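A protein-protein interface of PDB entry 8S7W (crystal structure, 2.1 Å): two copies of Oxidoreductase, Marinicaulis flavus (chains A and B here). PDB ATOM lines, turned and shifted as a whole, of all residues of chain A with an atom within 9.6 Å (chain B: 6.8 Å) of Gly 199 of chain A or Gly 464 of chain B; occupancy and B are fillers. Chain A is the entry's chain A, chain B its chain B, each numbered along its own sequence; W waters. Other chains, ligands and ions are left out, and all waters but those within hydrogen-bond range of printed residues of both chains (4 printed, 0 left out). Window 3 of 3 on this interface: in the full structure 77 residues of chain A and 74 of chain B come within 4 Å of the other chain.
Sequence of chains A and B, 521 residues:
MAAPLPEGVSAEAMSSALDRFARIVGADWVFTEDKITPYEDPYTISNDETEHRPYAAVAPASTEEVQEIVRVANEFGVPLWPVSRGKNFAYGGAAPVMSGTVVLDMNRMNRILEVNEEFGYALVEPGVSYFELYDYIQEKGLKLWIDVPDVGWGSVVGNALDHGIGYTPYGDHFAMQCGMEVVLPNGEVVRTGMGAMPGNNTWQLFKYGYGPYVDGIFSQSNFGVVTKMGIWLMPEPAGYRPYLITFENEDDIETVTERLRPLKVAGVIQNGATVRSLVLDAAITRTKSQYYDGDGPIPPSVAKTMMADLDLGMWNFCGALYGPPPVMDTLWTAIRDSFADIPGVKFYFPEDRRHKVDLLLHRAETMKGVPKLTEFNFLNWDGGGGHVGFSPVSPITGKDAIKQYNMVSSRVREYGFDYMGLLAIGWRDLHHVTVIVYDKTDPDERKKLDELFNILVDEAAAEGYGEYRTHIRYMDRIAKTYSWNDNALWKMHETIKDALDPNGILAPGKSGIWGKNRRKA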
ATOM      1  N   ARG A 191      -0.922  -2.224   0.857  1.00  0.00           N
ATOM      2  CA  ARG A 191       0.532  -1.996   0.702  1.00  0.00           C
ATOM      3  C   ARG A 191       1.173  -1.913   2.091  1.00  0.00           C
ATOM      4  O   ARG A 191       0.616  -1.244   3.007  1.00  0.00           O
ATOM      5  CB  ARG A 191       0.779  -0.739  -0.129  1.00  0.00           C
ATOM      6  CG  ARG A 191       0.301  -0.870  -1.564  1.00  0.00           C
ATOM      7  CD  ARG A 191       0.482   0.415  -2.354  1.00  0.00           C
ATOM      8  NE  ARG A 191       0.227   0.148  -3.761  1.00  0.00           N
ATOM      9  CZ  ARG A 191       0.443   1.008  -4.755  1.00  0.00           C
ATOM     10  NH1 ARG A 191       0.991   2.189  -4.512  1.00  0.00           N
ATOM     11  NH2 ARG A 191       0.213   0.637  -5.998  1.00  0.00           N
ATOM     12  N   MET A 194       6.021   2.206   4.037  1.00  0.00           N
ATOM     13  CA  MET A 194       5.719   3.620   3.683  1.00  0.00           C
ATOM     14  C   MET A 194       4.721   3.633   2.512  1.00  0.00           C
ATOM     15  O   MET A 194       4.053   4.642   2.319  1.00  0.00           O
ATOM     16  CB  MET A 194       7.008   4.366   3.333  1.00  0.00           C
ATOM     17  CG  MET A 194       8.055   4.319   4.454  1.00  0.00           C
ATOM     18  SD  MET A 194       7.464   4.861   6.089  1.00  0.00           S
ATOM     19  CE  MET A 194       6.695   6.431   5.745  1.00  0.00           C
ATOM     20  N   GLY A 195       4.525   2.500   1.829  1.00  0.00           N
ATOM     21  CA  GLY A 195       3.506   2.375   0.767  1.00  0.00           C
ATOM     22  C   GLY A 195       2.097   2.651   1.290  1.00  0.00           C
ATOM     23  O   GLY A 195       1.234   3.065   0.504  1.00  0.00           O
ATOM     24  N   ALA A 196       1.843   2.461   2.585  1.00  0.00           N
ATOM     25  CA  ALA A 196       0.524   2.762   3.177  1.00  0.00           C
ATOM     26  C   ALA A 196       0.298   4.280   3.231  1.00  0.00           C
ATOM     27  O   ALA A 196      -0.870   4.689   3.412  1.00  0.00           O
ATOM     28  CB  ALA A 196       0.426   2.122   4.535  1.00  0.00           C
ATOM     29  N   MET A 197       1.350   5.092   3.077  1.00  0.00           N
ATOM     30  CA  MET A 197       1.223   6.570   3.170  1.00  0.00           C
ATOM     31  C   MET A 197       1.023   7.159   1.785  1.00  0.00           C
ATOM     32  O   MET A 197       1.971   7.160   0.999  1.00  0.00           O
ATOM     33  CB  MET A 197       2.463   7.242   3.771  1.00  0.00           C
ATOM     34  CG  MET A 197       2.399   8.754   3.602  1.00  0.00           C
ATOM     35  SD  MET A 197       3.396   9.639   4.758  1.00  0.00           S
ATOM     36  CE  MET A 197       2.191   9.889   6.055  1.00  0.00           C
ATOM     37  N   PRO A 198      -0.129   7.800   1.493  1.00  0.00           N
ATOM     38  CA  PRO A 198      -0.349   8.412   0.179  1.00  0.00           C
ATOM     39  C   PRO A 198       0.685   9.531  -0.032  1.00  0.00           C
ATOM     40  O   PRO A 198       0.878  10.314   0.880  1.00  0.00           O
ATOM     41  CB  PRO A 198      -1.752   9.043   0.255  1.00  0.00           C
ATOM     42  CG  PRO A 198      -2.371   8.504   1.532  1.00  0.00           C
ATOM     43  CD  PRO A 198      -1.208   8.135   2.434  1.00  0.00           C
ATOM     44  N   GLY A 199       1.321   9.560  -1.196  1.00  0.00           N
ATOM     45  CA  GLY A 199       2.285  10.601  -1.604  1.00  0.00           C
ATOM     46  C   GLY A 199       3.703  10.319  -1.112  1.00  0.00           C
ATOM     47  O   GLY A 199       4.581  11.186  -1.307  1.00  0.00           O
ATOM     48  N   ASN A 200       3.951   9.144  -0.519  1.00  0.00           N
ATOM     49  CA  ASN A 200       5.301   8.808   0.002  1.00  0.00           C
ATOM     50  C   ASN A 200       6.257   8.721  -1.178  1.00  0.00           C
ATOM     51  O   ASN A 200       5.805   8.365  -2.255  1.00  0.00           O
ATOM     52  CB  ASN A 200       5.333   7.473   0.752  1.00  0.00           C
ATOM     53  CG  ASN A 200       5.307   6.321  -0.229  1.00  0.00           C
ATOM     54  OD1 ASN A 200       6.366   5.853  -0.669  1.00  0.00           O
ATOM     55  ND2 ASN A 200       4.100   5.939  -0.645  1.00  0.00           N
ATOM     56  N   ASN A 201       7.544   8.924  -0.944  1.00  0.00           N
ATOM     57  CA  ASN A 201       8.619   8.590  -1.923  1.00  0.00           C
ATOM     58  C   ASN A 201       9.595   7.626  -1.238  1.00  0.00           C
ATOM     59  O   ASN A 201      10.781   7.629  -1.584  1.00  0.00           O
ATOM     60  CB  ASN A 201       9.266   9.874  -2.464  1.00  0.00           C
ATOM     61  CG  ASN A 201       8.338  10.630  -3.400  1.00  0.00           C
ATOM     62  OD1 ASN A 201       7.701  11.611  -3.017  1.00  0.00           O
ATOM     63  ND2 ASN A 201       8.148  10.106  -4.591  1.00  0.00           N
ATOM     64  N   THR A 202       9.128   6.847  -0.259  1.00  0.00           N
ATOM     65  CA  THR A 202      10.019   6.111   0.676  1.00  0.00           C
ATOM     66  C   THR A 202       9.657   4.618   0.758  1.00  0.00           C
ATOM     67  O   THR A 202      10.307   3.921   1.555  1.00  0.00           O
ATOM     68  CB  THR A 202       9.950   6.776   2.053  1.00  0.00           C
ATOM     69  OG1 THR A 202       8.560   6.976   2.332  1.00  0.00           O
ATOM     70  CG2 THR A 202      10.736   8.080   2.103  1.00  0.00           C
ATOM     71  N   TRP A 203       8.686   4.145  -0.034  1.00  0.00           N
ATOM     72  CA  TRP A 203       8.248   2.723  -0.070  1.00  0.00           C
ATOM     73  C   TRP A 203       9.453   1.784  -0.173  1.00  0.00           C
ATOM     74  O   TRP A 203       9.450   0.750   0.513  1.00  0.00           O
ATOM     75  CB  TRP A 203       7.285   2.486  -1.228  1.00  0.00           C
ATOM     76  CG  TRP A 203       6.399   1.290  -1.083  1.00  0.00           C
ATOM     77  CD1 TRP A 203       6.177   0.532   0.035  1.00  0.00           C
ATOM     78  CD2 TRP A 203       5.561   0.742  -2.120  1.00  0.00           C
ATOM     79  NE1 TRP A 203       5.243  -0.437  -0.237  1.00  0.00           N
ATOM     80  CE2 TRP A 203       4.866  -0.352  -1.553  1.00  0.00           C
ATOM     81  CE3 TRP A 203       5.329   1.071  -3.461  1.00  0.00           C
ATOM     82  CZ2 TRP A 203       3.941  -1.108  -2.284  1.00  0.00           C
ATOM     83  CZ3 TRP A 203       4.407   0.333  -4.183  1.00  0.00           C
ATOM     84  CH2 TRP A 203       3.734  -0.747  -3.598  1.00  0.00           C
ATOM     85  N   LEU A 205      12.688   2.709   0.592  1.00  0.00           N
ATOM     86  CA  LEU A 205      13.836   3.302   1.328  1.00  0.00           C
ATOM     87  C   LEU A 205      13.821   2.887   2.815  1.00  0.00           C
ATOM     88  O   LEU A 205      14.888   2.976   3.433  1.00  0.00           O
ATOM     89  CB  LEU A 205      13.820   4.836   1.209  1.00  0.00           C
ATOM     90  CG  LEU A 205      13.801   5.430  -0.202  1.00  0.00           C
ATOM     91  CD1 LEU A 205      13.895   6.946  -0.121  1.00  0.00           C
ATOM     92  CD2 LEU A 205      14.924   4.882  -1.060  1.00  0.00           C
ATOM     93  N   VAL B 393      10.099   9.779   8.074  1.00  0.00           N
ATOM     94  CA  VAL B 393      11.031   9.205   7.064  1.00  0.00           C
ATOM     95  C   VAL B 393      10.935  10.008   5.763  1.00  0.00           C
ATOM     96  O   VAL B 393       9.814  10.293   5.325  1.00  0.00           O
ATOM     97  CB  VAL B 393      10.673   7.733   6.773  1.00  0.00           C
ATOM     98  CG1 VAL B 393      11.732   7.070   5.929  1.00  0.00           C
ATOM     99  CG2 VAL B 393      10.446   6.957   8.048  1.00  0.00           C
ATOM    100  N   SER B 394      12.053  10.227   5.096  1.00  0.00           N
ATOM    101  CA  SER B 394      12.125  10.985   3.818  1.00  0.00           C
ATOM    102  C   SER B 394      13.266  10.414   2.990  1.00  0.00           C
ATOM    103  O   SER B 394      14.096   9.698   3.552  1.00  0.00           O
ATOM    104  CB  SER B 394      12.322  12.480   4.082  1.00  0.00           C
ATOM    105  OG  SER B 394      13.500  12.679   4.848  1.00  0.00           O
ATOM    106  N   PRO B 395      13.331  10.696   1.663  1.00  0.00           N
ATOM    107  CA  PRO B 395      14.506  10.363   0.867  1.00  0.00           C
ATOM    108  C   PRO B 395      15.741  11.161   1.305  1.00  0.00           C
ATOM    109  O   PRO B 395      15.568  12.271   1.795  1.00  0.00           O
ATOM    110  CB  PRO B 395      14.102  10.675  -0.591  1.00  0.00           C
ATOM    111  CG  PRO B 395      12.567  10.777  -0.555  1.00  0.00           C
ATOM    112  CD  PRO B 395      12.241  11.271   0.844  1.00  0.00           C
ATOM    113  N   GLU B 459       1.685  18.781   8.460  1.00  0.00           N
ATOM    114  CA  GLU B 459       2.556  19.426   7.453  1.00  0.00           C
ATOM    115  C   GLU B 459       3.511  18.368   6.886  1.00  0.00           C
ATOM    116  O   GLU B 459       3.854  18.450   5.678  1.00  0.00           O
ATOM    117  CB  GLU B 459       3.304  20.615   8.054  1.00  0.00           C
ATOM    118  CG  GLU B 459       2.388  21.762   8.410  1.00  0.00           C
ATOM    119  CD  GLU B 459       3.086  23.091   8.689  1.00  0.00           C
ATOM    120  OE1 GLU B 459       4.262  23.097   9.075  1.00  0.00           O
ATOM    121  OE2 GLU B 459       2.441  24.114   8.494  1.00  0.00           O
ATOM    122  N   ALA B 460       3.954  17.423   7.716  1.00  0.00           N
ATOM    123  CA  ALA B 460       4.896  16.375   7.272  1.00  0.00           C
ATOM    124  C   ALA B 460       4.159  15.410   6.324  1.00  0.00           C
ATOM    125  O   ALA B 460       4.690  15.109   5.236  1.00  0.00           O
ATOM    126  CB  ALA B 460       5.514  15.695   8.462  1.00  0.00           C
ATOM    127  N   ALA B 461       2.960  14.988   6.688  1.00  0.00           N
ATOM    128  CA  ALA B 461       2.127  14.020   5.930  1.00  0.00           C
ATOM    129  C   ALA B 461       1.727  14.628   4.577  1.00  0.00           C
ATOM    130  O   ALA B 461       1.683  13.875   3.572  1.00  0.00           O
ATOM    131  CB  ALA B 461       0.907  13.652   6.736  1.00  0.00           C
ATOM    132  N   ALA B 462       1.491  15.946   4.528  1.00  0.00           N
ATOM    133  CA  ALA B 462       1.136  16.674   3.281  1.00  0.00           C
ATOM    134  C   ALA B 462       2.295  16.550   2.297  1.00  0.00           C
ATOM    135  O   ALA B 462       2.028  16.600   1.086  1.00  0.00           O
ATOM    136  CB  ALA B 462       0.806  18.125   3.558  1.00  0.00           C
ATOM    137  N   GLU B 463       3.533  16.404   2.785  1.00  0.00           N
ATOM    138  CA  GLU B 463       4.738  16.209   1.932  1.00  0.00           C
ATOM    139  C   GLU B 463       4.995  14.709   1.666  1.00  0.00           C
ATOM    140  O   GLU B 463       5.946  14.408   0.934  1.00  0.00           O
ATOM    141  CB  GLU B 463       5.976  16.816   2.596  1.00  0.00           C
ATOM    142  CG  GLU B 463       5.849  18.293   2.898  1.00  0.00           C
ATOM    143  CD  GLU B 463       5.585  19.141   1.661  1.00  0.00           C
ATOM    144  OE1 GLU B 463       6.370  19.026   0.687  1.00  0.00           O
ATOM    145  OE2 GLU B 463       4.587  19.879   1.667  1.00  0.00           O
ATOM    146  N   GLY B 464       4.242  13.801   2.272  1.00  0.00           N
ATOM    147  CA  GLY B 464       4.489  12.342   2.153  1.00  0.00           C
ATOM    148  C   GLY B 464       5.605  11.848   3.079  1.00  0.00           C
ATOM    149  O   GLY B 464       6.325  10.895   2.725  1.00  0.00           O
ATOM    150  N   TYR B 465       5.773  12.508   4.217  1.00  0.00           N
ATOM    151  CA  TYR B 465       6.736  12.138   5.280  1.00  0.00           C
ATOM    152  C   TYR B 465       5.944  11.543   6.436  1.00  0.00           C
ATOM    153  O   TYR B 465       5.157  12.270   7.050  1.00  0.00           O
ATOM    154  CB  TYR B 465       7.530  13.352   5.771  1.00  0.00           C
ATOM    155  CG  TYR B 465       8.267  14.135   4.709  1.00  0.00           C
ATOM    156  CD1 TYR B 465       8.858  13.522   3.613  1.00  0.00           C
ATOM    157  CD2 TYR B 465       8.419  15.512   4.838  1.00  0.00           C
ATOM    158  CE1 TYR B 465       9.547  14.261   2.656  1.00  0.00           C
ATOM    159  CE2 TYR B 465       9.116  16.261   3.904  1.00  0.00           C
ATOM    160  CZ  TYR B 465       9.682  15.637   2.810  1.00  0.00           C
ATOM    161  OH  TYR B 465      10.383  16.398   1.924  1.00  0.00           O
ATOM    162  N   GLY B 466       6.155  10.253   6.699  1.00  0.00           N
ATOM    163  CA  GLY B 466       5.422   9.488   7.723  1.00  0.00           C
ATOM    164  C   GLY B 466       6.304   9.126   8.903  1.00  0.00           C
ATOM    165  O   GLY B 466       7.489   8.763   8.706  1.00  0.00           O
ATOM    166  N   TRP B 484      -3.598   4.707   2.732  1.00  0.00           N
ATOM    167  CA  TRP B 484      -3.718   4.174   1.348  1.00  0.00           C
ATOM    168  C   TRP B 484      -4.865   3.157   1.292  1.00  0.00           C
ATOM    169  O   TRP B 484      -4.934   2.251   2.166  1.00  0.00           O
ATOM    170  CB  TRP B 484      -2.413   3.588   0.801  1.00  0.00           C
ATOM    171  CG  TRP B 484      -2.497   3.239  -0.658  1.00  0.00           C
ATOM    172  CD1 TRP B 484      -2.352   4.096  -1.716  1.00  0.00           C
ATOM    173  CD2 TRP B 484      -2.766   1.949  -1.233  1.00  0.00           C
ATOM    174  NE1 TRP B 484      -2.501   3.429  -2.905  1.00  0.00           N
ATOM    175  CE2 TRP B 484      -2.778   2.113  -2.642  1.00  0.00           C
ATOM    176  CE3 TRP B 484      -3.012   0.683  -0.700  1.00  0.00           C
ATOM    177  CZ2 TRP B 484      -2.980   1.053  -3.522  1.00  0.00           C
ATOM    178  CZ3 TRP B 484      -3.272  -0.350  -1.573  1.00  0.00           C
ATOM    179  CH2 TRP B 484      -3.220  -0.176  -2.964  1.00  0.00           C
HETATM  180  O   HOH W   1       7.841   8.957   4.021  1.00  0.00           O
HETATM  181  O   HOH W   2       8.672  10.656   0.958  1.00  0.00           O
HETATM  182  O   HOH W   3       0.271  11.659   3.133  1.00  0.00           O
HETATM  183  O   HOH W   4       8.034  12.756  -0.215  1.00  0.00           O
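Along chain B the printed residues that touch a printed residue of chain A span positions 394 to 484. Printed residues of chain A that touch a printed residue of chain B: Arg 191, Met 194, Gly 195, Ala 196, Met 197, Gly 199, Asn 200, Asn 201, Thr 202 and Leu 205. Hydrophobic or aromatic side chains of chain A that line the printed part of chain B: Met 194, Met 197 and Leu 205.
Gly 199 of chain A touches just one residue of chain B: Gly 464. Of the printed residues of chain B, Asn 200 of chain A touches Gly 464. Of the printed residues of chain B, Asn 201 of chain A touches Pro 395. Of the printed residues of chain B, Leu 205 of chain A touches Pro 395. Of the printed residues of chain A, Ser 394 of chain B touches Thr 202. Ala 462 of chain B touches none of the printed residues of chain A. Gly 464 of chain B touches just these residues of chain A: Met 197, Gly 199 and Asn 200. The nearest printed residue of chain A that does not touch Gly 464 of chain B is Pro 198 of chain A (4.3 Å). The nearest printed residue of chain B that does not touch Arg 191 of chain A is Gly 464 of chain B (12.5 Å).
O of Gly 464 of chain B lies close to SD of Met 197 of chain A, 3.8 Å away. The backbone NH (N) of Tyr 465 of chain B lies close to the side-chain sulfur (SD) of Met 197 of chain A (3.8 Å). The backbone carbonyl oxygen (O) of Ala 196 of chain A lies within hydrogen-bond range of the backbone NH (N) of Trp 484 of chain B (2.8 Å). The side-chain sulfur (SD) of Met 197 of chain A sits at hydrogen-bond distance from the backbone NH (N) of Gly 466 of chain B (3.4 Å).
NE of Arg 191 of chain A touches CZ2 of Trp 484 of chain B, at 3.3 Å. Met 194 of chain A touches Gly 466 of chain B. Trp 484 of chain B touches Gly 195 of chain A (CB to O, 3.7 Å). Gly 464 of chain B touches Gly 199 of chain A (CA to O, 3.6 Å). Asn 200 of chain A touches Gly 464 of chain B. Asn 201 of chain A touches Pro 395 of chain B (O to CG, 3.8 Å). Thr 202 of chain A touches Ser 394 of chain B. N of Pro 395 of chain B touches CG2 of Thr 202 of chain A (3.7 Å). CD1 of Leu 205 of chain A touches CA of Pro 395 of chain B, at 3.6 Å.
No position is printed for both chains. Of the 13 pairs that touch across the chains among the printed residues, none has its exchanged pair printed and touching as well.
O of Ala 460 of chain B is in hydrogen-bond range of N of Tyr 465 of chain B (3.0 Å). The backbone carbonyl oxygen (O) of Met 197 of chain A is in hydrogen-bond range of the side-chain amide nitrogen (ND2) of Asn 200 of chain A (3.0 Å). The backbone NH (N) of Trp 203 of chain A lies within hydrogen-bond range of the side-chain amide oxygen (OD1) of Asn 200 of chain A (3.0 Å). The backbone NH of Thr 202 of chain A sits at hydrogen-bond distance from the side-chain amide oxygen of Asn 200 of chain A (3.0 Å). The backbone carbonyl oxygen (O) of Gly 466 of chain B lies within hydrogen-bond range of the backbone NH (N) of Val 393 of chain B, at 2.9 Å. The side-chain amide nitrogen of Asn 200 of chain A is in hydrogen-bond range of the backbone carbonyl oxygen of Met 194 of chain A (3.2 Å).
Water W3 bridges O of Ala 461 of chain B (2.7 Å) and O of Pro 198 of chain A (2.7 Å). Water W1 lies within hydrogen-bond range of OG1 of Thr 202 of chain A (2.7 Å), O of Val 393 of chain B (2.7 Å), O of Gly 464 of chain B (2.8 Å) and N of Gly 466 of chain B (3.4 Å). Water W2 lies within hydrogen-bond range of the backbone NH of Asn 201 of chain A and the backbone carbonyl oxygen of Gly 464 of chain B. Water W4 lies within hydrogen-bond range of O of Glu 463 of chain B (2.9 Å) and OD1 of Asn 201 of chain A (3.0 Å).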
